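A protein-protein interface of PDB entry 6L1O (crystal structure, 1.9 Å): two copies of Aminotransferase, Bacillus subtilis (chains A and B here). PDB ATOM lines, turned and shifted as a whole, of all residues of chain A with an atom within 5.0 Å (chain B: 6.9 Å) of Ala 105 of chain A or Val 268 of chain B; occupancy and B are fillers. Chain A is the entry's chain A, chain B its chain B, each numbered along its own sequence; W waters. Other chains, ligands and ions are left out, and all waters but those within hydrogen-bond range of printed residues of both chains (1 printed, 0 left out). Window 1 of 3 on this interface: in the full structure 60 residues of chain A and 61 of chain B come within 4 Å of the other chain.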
ATOM      1  N   PHE A 100      26.638   5.815 -11.383  1.00  0.00           N
ATOM      2  CA  PHE A 100      25.753   6.671 -10.616  1.00  0.00           C
ATOM      3  C   PHE A 100      26.411   7.065  -9.279  1.00  0.00           C
ATOM      4  O   PHE A 100      27.192   6.301  -8.742  1.00  0.00           O
ATOM      5  CB  PHE A 100      24.477   5.894 -10.248  1.00  0.00           C
ATOM      6  CG  PHE A 100      23.594   5.553 -11.401  1.00  0.00           C
ATOM      7  CD1 PHE A 100      23.108   6.543 -12.231  1.00  0.00           C
ATOM      8  CD2 PHE A 100      23.263   4.251 -11.664  1.00  0.00           C
ATOM      9  CE1 PHE A 100      22.266   6.225 -13.290  1.00  0.00           C
ATOM     10  CE2 PHE A 100      22.446   3.921 -12.733  1.00  0.00           C
ATOM     11  CZ  PHE A 100      21.925   4.933 -13.529  1.00  0.00           C
ATOM     12  N   GLY A 101      26.035   8.209  -8.738  1.00  0.00           N
ATOM     13  CA  GLY A 101      26.425   8.595  -7.389  1.00  0.00           C
ATOM     14  C   GLY A 101      25.527   7.935  -6.347  1.00  0.00           C
ATOM     15  O   GLY A 101      24.794   8.632  -5.624  1.00  0.00           O
ATOM     16  N   GLY A 102      25.542   6.602  -6.329  1.00  0.00           N
ATOM     17  CA  GLY A 102      24.745   5.791  -5.393  1.00  0.00           C
ATOM     18  C   GLY A 102      23.443   5.303  -6.011  1.00  0.00           C
ATOM     19  O   GLY A 102      22.926   5.878  -6.965  1.00  0.00           O
ATOM     20  N   GLY A 103      22.938   4.200  -5.494  1.00  0.00           N
ATOM     21  CA  GLY A 103      21.696   3.592  -6.015  1.00  0.00           C
ATOM     22  C   GLY A 103      20.527   4.538  -5.989  1.00  0.00           C
ATOM     23  O   GLY A 103      19.717   4.536  -6.876  1.00  0.00           O
ATOM     24  N   LYS A 104      20.428   5.343  -4.952  1.00  0.00           N
ATOM     25  CA  LYS A 104      19.363   6.313  -4.823  1.00  0.00           C
ATOM     26  C   LYS A 104      19.323   7.278  -6.042  1.00  0.00           C
ATOM     27  O   LYS A 104      18.268   7.540  -6.622  1.00  0.00           O
ATOM     28  CB  LYS A 104      19.566   7.086  -3.522  1.00  0.00           C
ATOM     29  CG  LYS A 104      18.420   7.968  -3.103  1.00  0.00           C
ATOM     30  CD  LYS A 104      18.675   8.425  -1.639  1.00  0.00           C
ATOM     31  CE  LYS A 104      17.403   8.753  -0.918  1.00  0.00           C
ATOM     32  NZ  LYS A 104      17.725   9.219   0.472  1.00  0.00           N
ATOM     33  N   ALA A 105      20.471   7.814  -6.416  1.00  0.00           N
ATOM     34  CA  ALA A 105      20.579   8.641  -7.663  1.00  0.00           C
ATOM     35  C   ALA A 105      20.262   7.858  -8.923  1.00  0.00           C
ATOM     36  O   ALA A 105      19.565   8.372  -9.820  1.00  0.00           O
ATOM     37  CB  ALA A 105      21.954   9.283  -7.772  1.00  0.00           C
ATOM     38  N   GLY A 106      20.700   6.606  -8.984  1.00  0.00           N
ATOM     39  CA  GLY A 106      20.393   5.737 -10.083  1.00  0.00           C
ATOM     40  C   GLY A 106      18.902   5.511 -10.285  1.00  0.00           C
ATOM     41  O   GLY A 106      18.419   5.535 -11.415  1.00  0.00           O
ATOM     42  N   LEU A 107      18.177   5.304  -9.199  1.00  0.00           N
ATOM     43  CA  LEU A 107      16.725   5.138  -9.284  1.00  0.00           C
ATOM     44  C   LEU A 107      16.041   6.392  -9.786  1.00  0.00           C
ATOM     45  O   LEU A 107      15.041   6.318 -10.534  1.00  0.00           O
ATOM     46  CB  LEU A 107      16.108   4.746  -7.935  1.00  0.00           C
ATOM     47  CG  LEU A 107      16.500   3.404  -7.327  1.00  0.00           C
ATOM     48  CD1 LEU A 107      16.073   3.448  -5.856  1.00  0.00           C
ATOM     49  CD2 LEU A 107      15.816   2.298  -8.061  1.00  0.00           C
ATOM     50  N   TYR A 108      16.532   7.553  -9.409  1.00  0.00           N
ATOM     51  CA  TYR A 108      15.949   8.809  -9.889  1.00  0.00           C
ATOM     52  C   TYR A 108      16.201   8.967 -11.400  1.00  0.00           C
ATOM     53  O   TYR A 108      15.280   9.257 -12.160  1.00  0.00           O
ATOM     54  CB  TYR A 108      16.498  10.010  -9.130  1.00  0.00           C
ATOM     55  CG  TYR A 108      16.136  11.316  -9.758  1.00  0.00           C
ATOM     56  CD1 TYR A 108      14.861  11.857  -9.565  1.00  0.00           C
ATOM     57  CD2 TYR A 108      17.058  12.048 -10.521  1.00  0.00           C
ATOM     58  CE1 TYR A 108      14.488  13.044 -10.137  1.00  0.00           C
ATOM     59  CE2 TYR A 108      16.682  13.283 -11.112  1.00  0.00           C
ATOM     60  CZ  TYR A 108      15.391  13.763 -10.892  1.00  0.00           C
ATOM     61  OH  TYR A 108      14.979  14.926 -11.431  1.00  0.00           O
ATOM     62  N   VAL A 109      17.443   8.777 -11.803  1.00  0.00           N
ATOM     63  CA  VAL A 109      17.836   8.932 -13.244  1.00  0.00           C
ATOM     64  C   VAL A 109      17.067   7.929 -14.104  1.00  0.00           C
ATOM     65  O   VAL A 109      16.549   8.276 -15.158  1.00  0.00           O
ATOM     66  CB  VAL A 109      19.347   8.796 -13.412  1.00  0.00           C
ATOM     67  CG1 VAL A 109      19.767   8.764 -14.893  1.00  0.00           C
ATOM     68  CG2 VAL A 109      20.067   9.897 -12.656  1.00  0.00           C
ATOM     69  N   LEU A 110      16.958   6.688 -13.629  1.00  0.00           N
ATOM     70  CA  LEU A 110      16.345   5.646 -14.397  1.00  0.00           C
ATOM     71  C   LEU A 110      14.881   5.931 -14.602  1.00  0.00           C
ATOM     72  O   LEU A 110      14.401   5.822 -15.729  1.00  0.00           O
ATOM     73  CB  LEU A 110      16.565   4.267 -13.780  1.00  0.00           C
ATOM     74  CG  LEU A 110      17.959   3.648 -13.956  1.00  0.00           C
ATOM     75  CD1 LEU A 110      18.172   2.480 -12.984  1.00  0.00           C
ATOM     76  CD2 LEU A 110      18.171   3.194 -15.360  1.00  0.00           C
ATOM     77  N   MET A 137       8.218  12.106  -8.800  1.00  0.00           N
ATOM     78  CA  MET A 137       8.935  13.164  -9.479  1.00  0.00           C
ATOM     79  C   MET A 137       8.906  13.080 -10.987  1.00  0.00           C
ATOM     80  O   MET A 137       9.133  14.098 -11.639  1.00  0.00           O
ATOM     81  CB  MET A 137      10.392  13.217  -9.015  1.00  0.00           C
ATOM     82  CG  MET A 137      10.468  13.599  -7.543  1.00  0.00           C
ATOM     83  SD  MET A 137      12.101  13.183  -6.859  1.00  0.00           S
ATOM     84  CE  MET A 137      13.013  14.626  -7.373  1.00  0.00           C
ATOM     85  N   TYR B 108      21.073  22.124 -12.422  1.00  0.00           N
ATOM     86  CA  TYR B 108      19.962  21.207 -12.643  1.00  0.00           C
ATOM     87  C   TYR B 108      18.949  21.226 -11.474  1.00  0.00           C
ATOM     88  O   TYR B 108      17.737  21.356 -11.679  1.00  0.00           O
ATOM     89  CB  TYR B 108      20.425  19.792 -12.881  1.00  0.00           C
ATOM     90  CG  TYR B 108      19.332  18.777 -12.997  1.00  0.00           C
ATOM     91  CD1 TYR B 108      18.556  18.692 -14.177  1.00  0.00           C
ATOM     92  CD2 TYR B 108      18.965  17.959 -11.912  1.00  0.00           C
ATOM     93  CE1 TYR B 108      17.511  17.822 -14.286  1.00  0.00           C
ATOM     94  CE2 TYR B 108      17.906  17.060 -12.028  1.00  0.00           C
ATOM     95  CZ  TYR B 108      17.198  16.973 -13.209  1.00  0.00           C
ATOM     96  OH  TYR B 108      16.151  16.116 -13.327  1.00  0.00           O
ATOM     97  N   VAL B 109      19.443  21.081 -10.275  1.00  0.00           N
ATOM     98  CA  VAL B 109      18.580  20.927  -9.094  1.00  0.00           C
ATOM     99  C   VAL B 109      17.803  22.210  -8.851  1.00  0.00           C
ATOM    100  O   VAL B 109      16.611  22.169  -8.592  1.00  0.00           O
ATOM    101  CB  VAL B 109      19.391  20.528  -7.845  1.00  0.00           C
ATOM    102  CG1 VAL B 109      18.548  20.621  -6.586  1.00  0.00           C
ATOM    103  CG2 VAL B 109      19.926  19.108  -7.960  1.00  0.00           C
ATOM    104  N   GLU B 263      14.862  19.302   0.238  1.00  0.00           N
ATOM    105  CA  GLU B 263      13.755  18.358   0.151  1.00  0.00           C
ATOM    106  C   GLU B 263      13.922  17.537  -1.119  1.00  0.00           C
ATOM    107  O   GLU B 263      13.754  16.325  -1.094  1.00  0.00           O
ATOM    108  CB  GLU B 263      12.424  19.142   0.188  1.00  0.00           C
ATOM    109  CG  GLU B 263      12.200  19.667   1.614  1.00  0.00           C
ATOM    110  CD  GLU B 263      10.885  20.388   1.828  1.00  0.00           C
ATOM    111  OE1 GLU B 263      10.039  20.423   0.906  1.00  0.00           O
ATOM    112  OE2 GLU B 263      10.708  20.923   2.943  1.00  0.00           O
ATOM    113  N   PHE B 264      14.338  18.202  -2.216  1.00  0.00           N
ATOM    114  CA  PHE B 264      14.646  17.489  -3.451  1.00  0.00           C
ATOM    115  C   PHE B 264      15.781  16.479  -3.235  1.00  0.00           C
ATOM    116  O   PHE B 264      15.675  15.280  -3.596  1.00  0.00           O
ATOM    117  CB  PHE B 264      15.051  18.486  -4.543  1.00  0.00           C
ATOM    118  CG  PHE B 264      15.194  17.882  -5.916  1.00  0.00           C
ATOM    119  CD1 PHE B 264      14.179  18.073  -6.889  1.00  0.00           C
ATOM    120  CD2 PHE B 264      16.351  17.196  -6.274  1.00  0.00           C
ATOM    121  CE1 PHE B 264      14.336  17.546  -8.156  1.00  0.00           C
ATOM    122  CE2 PHE B 264      16.508  16.657  -7.545  1.00  0.00           C
ATOM    123  CZ  PHE B 264      15.498  16.833  -8.488  1.00  0.00           C
ATOM    124  N   GLN B 265      16.905  16.972  -2.733  1.00  0.00           N
ATOM    125  CA  GLN B 265      18.095  16.162  -2.612  1.00  0.00           C
ATOM    126  C   GLN B 265      17.940  15.037  -1.598  1.00  0.00           C
ATOM    127  O   GLN B 265      18.563  13.965  -1.739  1.00  0.00           O
ATOM    128  CB  GLN B 265      19.299  17.052  -2.293  1.00  0.00           C
ATOM    129  CG  GLN B 265      19.598  18.018  -3.457  1.00  0.00           C
ATOM    130  CD  GLN B 265      21.053  18.489  -3.538  1.00  0.00           C
ATOM    131  OE1 GLN B 265      21.744  18.248  -4.560  1.00  0.00           O
ATOM    132  NE2 GLN B 265      21.521  19.105  -2.483  1.00  0.00           N
ATOM    133  N   ASP B 266      17.131  15.266  -0.556  1.00  0.00           N
ATOM    134  CA  ASP B 266      16.753  14.167   0.331  1.00  0.00           C
ATOM    135  C   ASP B 266      16.294  12.909  -0.387  1.00  0.00           C
ATOM    136  O   ASP B 266      16.627  11.803   0.007  1.00  0.00           O
ATOM    137  CB  ASP B 266      15.657  14.611   1.301  1.00  0.00           C
ATOM    138  CG  ASP B 266      16.165  15.507   2.428  1.00  0.00           C
ATOM    139  OD1 ASP B 266      17.405  15.723   2.576  1.00  0.00           O
ATOM    140  OD2 ASP B 266      15.299  16.027   3.160  1.00  0.00           O
ATOM    141  N   HIS B 267      15.542  13.086  -1.474  1.00  0.00           N
ATOM    142  CA  HIS B 267      15.056  11.952  -2.228  1.00  0.00           C
ATOM    143  C   HIS B 267      15.983  11.384  -3.289  1.00  0.00           C
ATOM    144  O   HIS B 267      15.754  10.295  -3.756  1.00  0.00           O
ATOM    145  CB  HIS B 267      13.733  12.348  -2.899  1.00  0.00           C
ATOM    146  CG  HIS B 267      12.636  12.596  -1.925  1.00  0.00           C
ATOM    147  ND1 HIS B 267      11.678  11.651  -1.618  1.00  0.00           N
ATOM    148  CD2 HIS B 267      12.359  13.677  -1.160  1.00  0.00           C
ATOM    149  CE1 HIS B 267      10.839  12.153  -0.735  1.00  0.00           C
ATOM    150  NE2 HIS B 267      11.228  13.380  -0.440  1.00  0.00           N
ATOM    151  N   VAL B 268      17.039  12.121  -3.667  1.00  0.00           N
ATOM    152  CA  VAL B 268      17.798  11.812  -4.850  1.00  0.00           C
ATOM    153  C   VAL B 268      19.311  11.822  -4.648  1.00  0.00           C
ATOM    154  O   VAL B 268      19.952  10.836  -4.894  1.00  0.00           O
ATOM    155  CB  VAL B 268      17.390  12.845  -5.940  1.00  0.00           C
ATOM    156  CG1 VAL B 268      18.214  12.719  -7.188  1.00  0.00           C
ATOM    157  CG2 VAL B 268      15.925  12.694  -6.299  1.00  0.00           C
ATOM    158  N   PHE B 269      19.851  12.988  -4.290  1.00  0.00           N
ATOM    159  CA  PHE B 269      21.320  13.270  -4.301  1.00  0.00           C
ATOM    160  C   PHE B 269      21.740  13.612  -2.867  1.00  0.00           C
ATOM    161  O   PHE B 269      21.842  14.808  -2.496  1.00  0.00           O
ATOM    162  CB  PHE B 269      21.655  14.481  -5.187  1.00  0.00           C
ATOM    163  CG  PHE B 269      21.296  14.331  -6.614  1.00  0.00           C
ATOM    164  CD1 PHE B 269      21.554  13.137  -7.292  1.00  0.00           C
ATOM    165  CD2 PHE B 269      20.712  15.397  -7.319  1.00  0.00           C
ATOM    166  CE1 PHE B 269      21.202  12.987  -8.644  1.00  0.00           C
ATOM    167  CE2 PHE B 269      20.363  15.266  -8.687  1.00  0.00           C
ATOM    168  CZ  PHE B 269      20.597  14.053  -9.349  1.00  0.00           C
ATOM    169  N   VAL B 270      21.903  12.602  -2.052  1.00  0.00           N
ATOM    170  CA  VAL B 270      22.299  12.816  -0.658  1.00  0.00           C
ATOM    171  C   VAL B 270      23.786  13.147  -0.534  1.00  0.00           C
ATOM    172  O   VAL B 270      24.564  12.972  -1.501  1.00  0.00           O
ATOM    173  CB  VAL B 270      21.954  11.626   0.238  1.00  0.00           C
ATOM    174  CG1 VAL B 270      20.434  11.417   0.254  1.00  0.00           C
ATOM    175  CG2 VAL B 270      22.699  10.368  -0.150  1.00  0.00           C
HETATM  176  O   HOH W   1      22.204   9.710  -3.799  1.00  0.00           O
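Of chain B, only Val 268 and Phe 269 come within 4 Å of Ala 105 of chain A. Gly 106 of chain A touches none of the printed residues of chain B. Printed residues of chain B within 4 Å of Tyr 108 of chain A: Tyr 108, Phe 264 and Val 268. Of the printed residues of chain B, Met 137 of chain A touches Phe 264 and Val 268. Of the printed residues of chain A, Phe 264 of chain B touches Tyr 108 and Met 137. Of the printed residues of chain A, Phe 269 of chain B touches Ala 105 (3.9 Å). Printed residues of chain A within 4 Å of Val 270 of chain B: Lys 104 (3.5 Å).
Tyr 108 of chain A touches its own counterpart, Tyr 108 of chain B. Positions printed for both chains: 108 and 109. Of the 11 pairs that touch across the chains among the printed residues, 1 has its exchanged pair printed and touching as well.
Water W1 lies within hydrogen-bond range of O of Val 268 of chain B (2.7 Å), O of Gly 101 of chain A (3.3 Å) and N of Val 270 of chain B (3.4 Å).
Among the printed residues, pairs that only touch across the chains: Met 137 of chain A with Phe 264 of chain B (3.3 Å), Lys 104 of chain A with Val 270 of chain B (3.5 Å), Tyr 108 of chain A with Val 268 of chain B (3.5 Å), Tyr 108 of chain A with Phe 264 of chain B (3.5 Å), Lys 104 of chain A with His 267 of chain B (3.6 Å), Met 137 of chain A with Val 268 of chain B (3.7 Å), Lys 104 of chain A with Val 268 of chain B (3.7 Å) and Ala 105 of chain A with Phe 269 of chain B (3.9 Å).
Printed residues of chain B that touch a printed residue of chain A: Tyr 108, Phe 264, Asp 266, His 267, Val 268, Phe 269 and Val 270. Hydrophobic or aromatic side chains of chain B that line the printed part of chain A: Tyr 108, Phe 264, Val 268, Phe 269 and Val 270. Hydrophobic or aromatic side chains of chain A within 4 Å of the printed part of chain B: Ala 105, Tyr 108 and Met 137. Among the printed residues, no Asp or Glu carboxylate lies within 4 Å of a Lys or Arg side-chain nitrogen of the other chain.
The side-chain hydroxyl of Tyr 108 of chain B lies within hydrogen-bond range of the side-chain hydroxyl of Tyr 108 of chain A, at 2.5 Å. The backbone carbonyl oxygen (O) of Asp 266 of chain B is in hydrogen-bond range of the side-chain amino group (NZ) of Lys 104 of chain A (2.8 Å). O of Val 268 of chain B lies within hydrogen-bond range of N of Ala 105 of chain A, 3.4 Å away.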
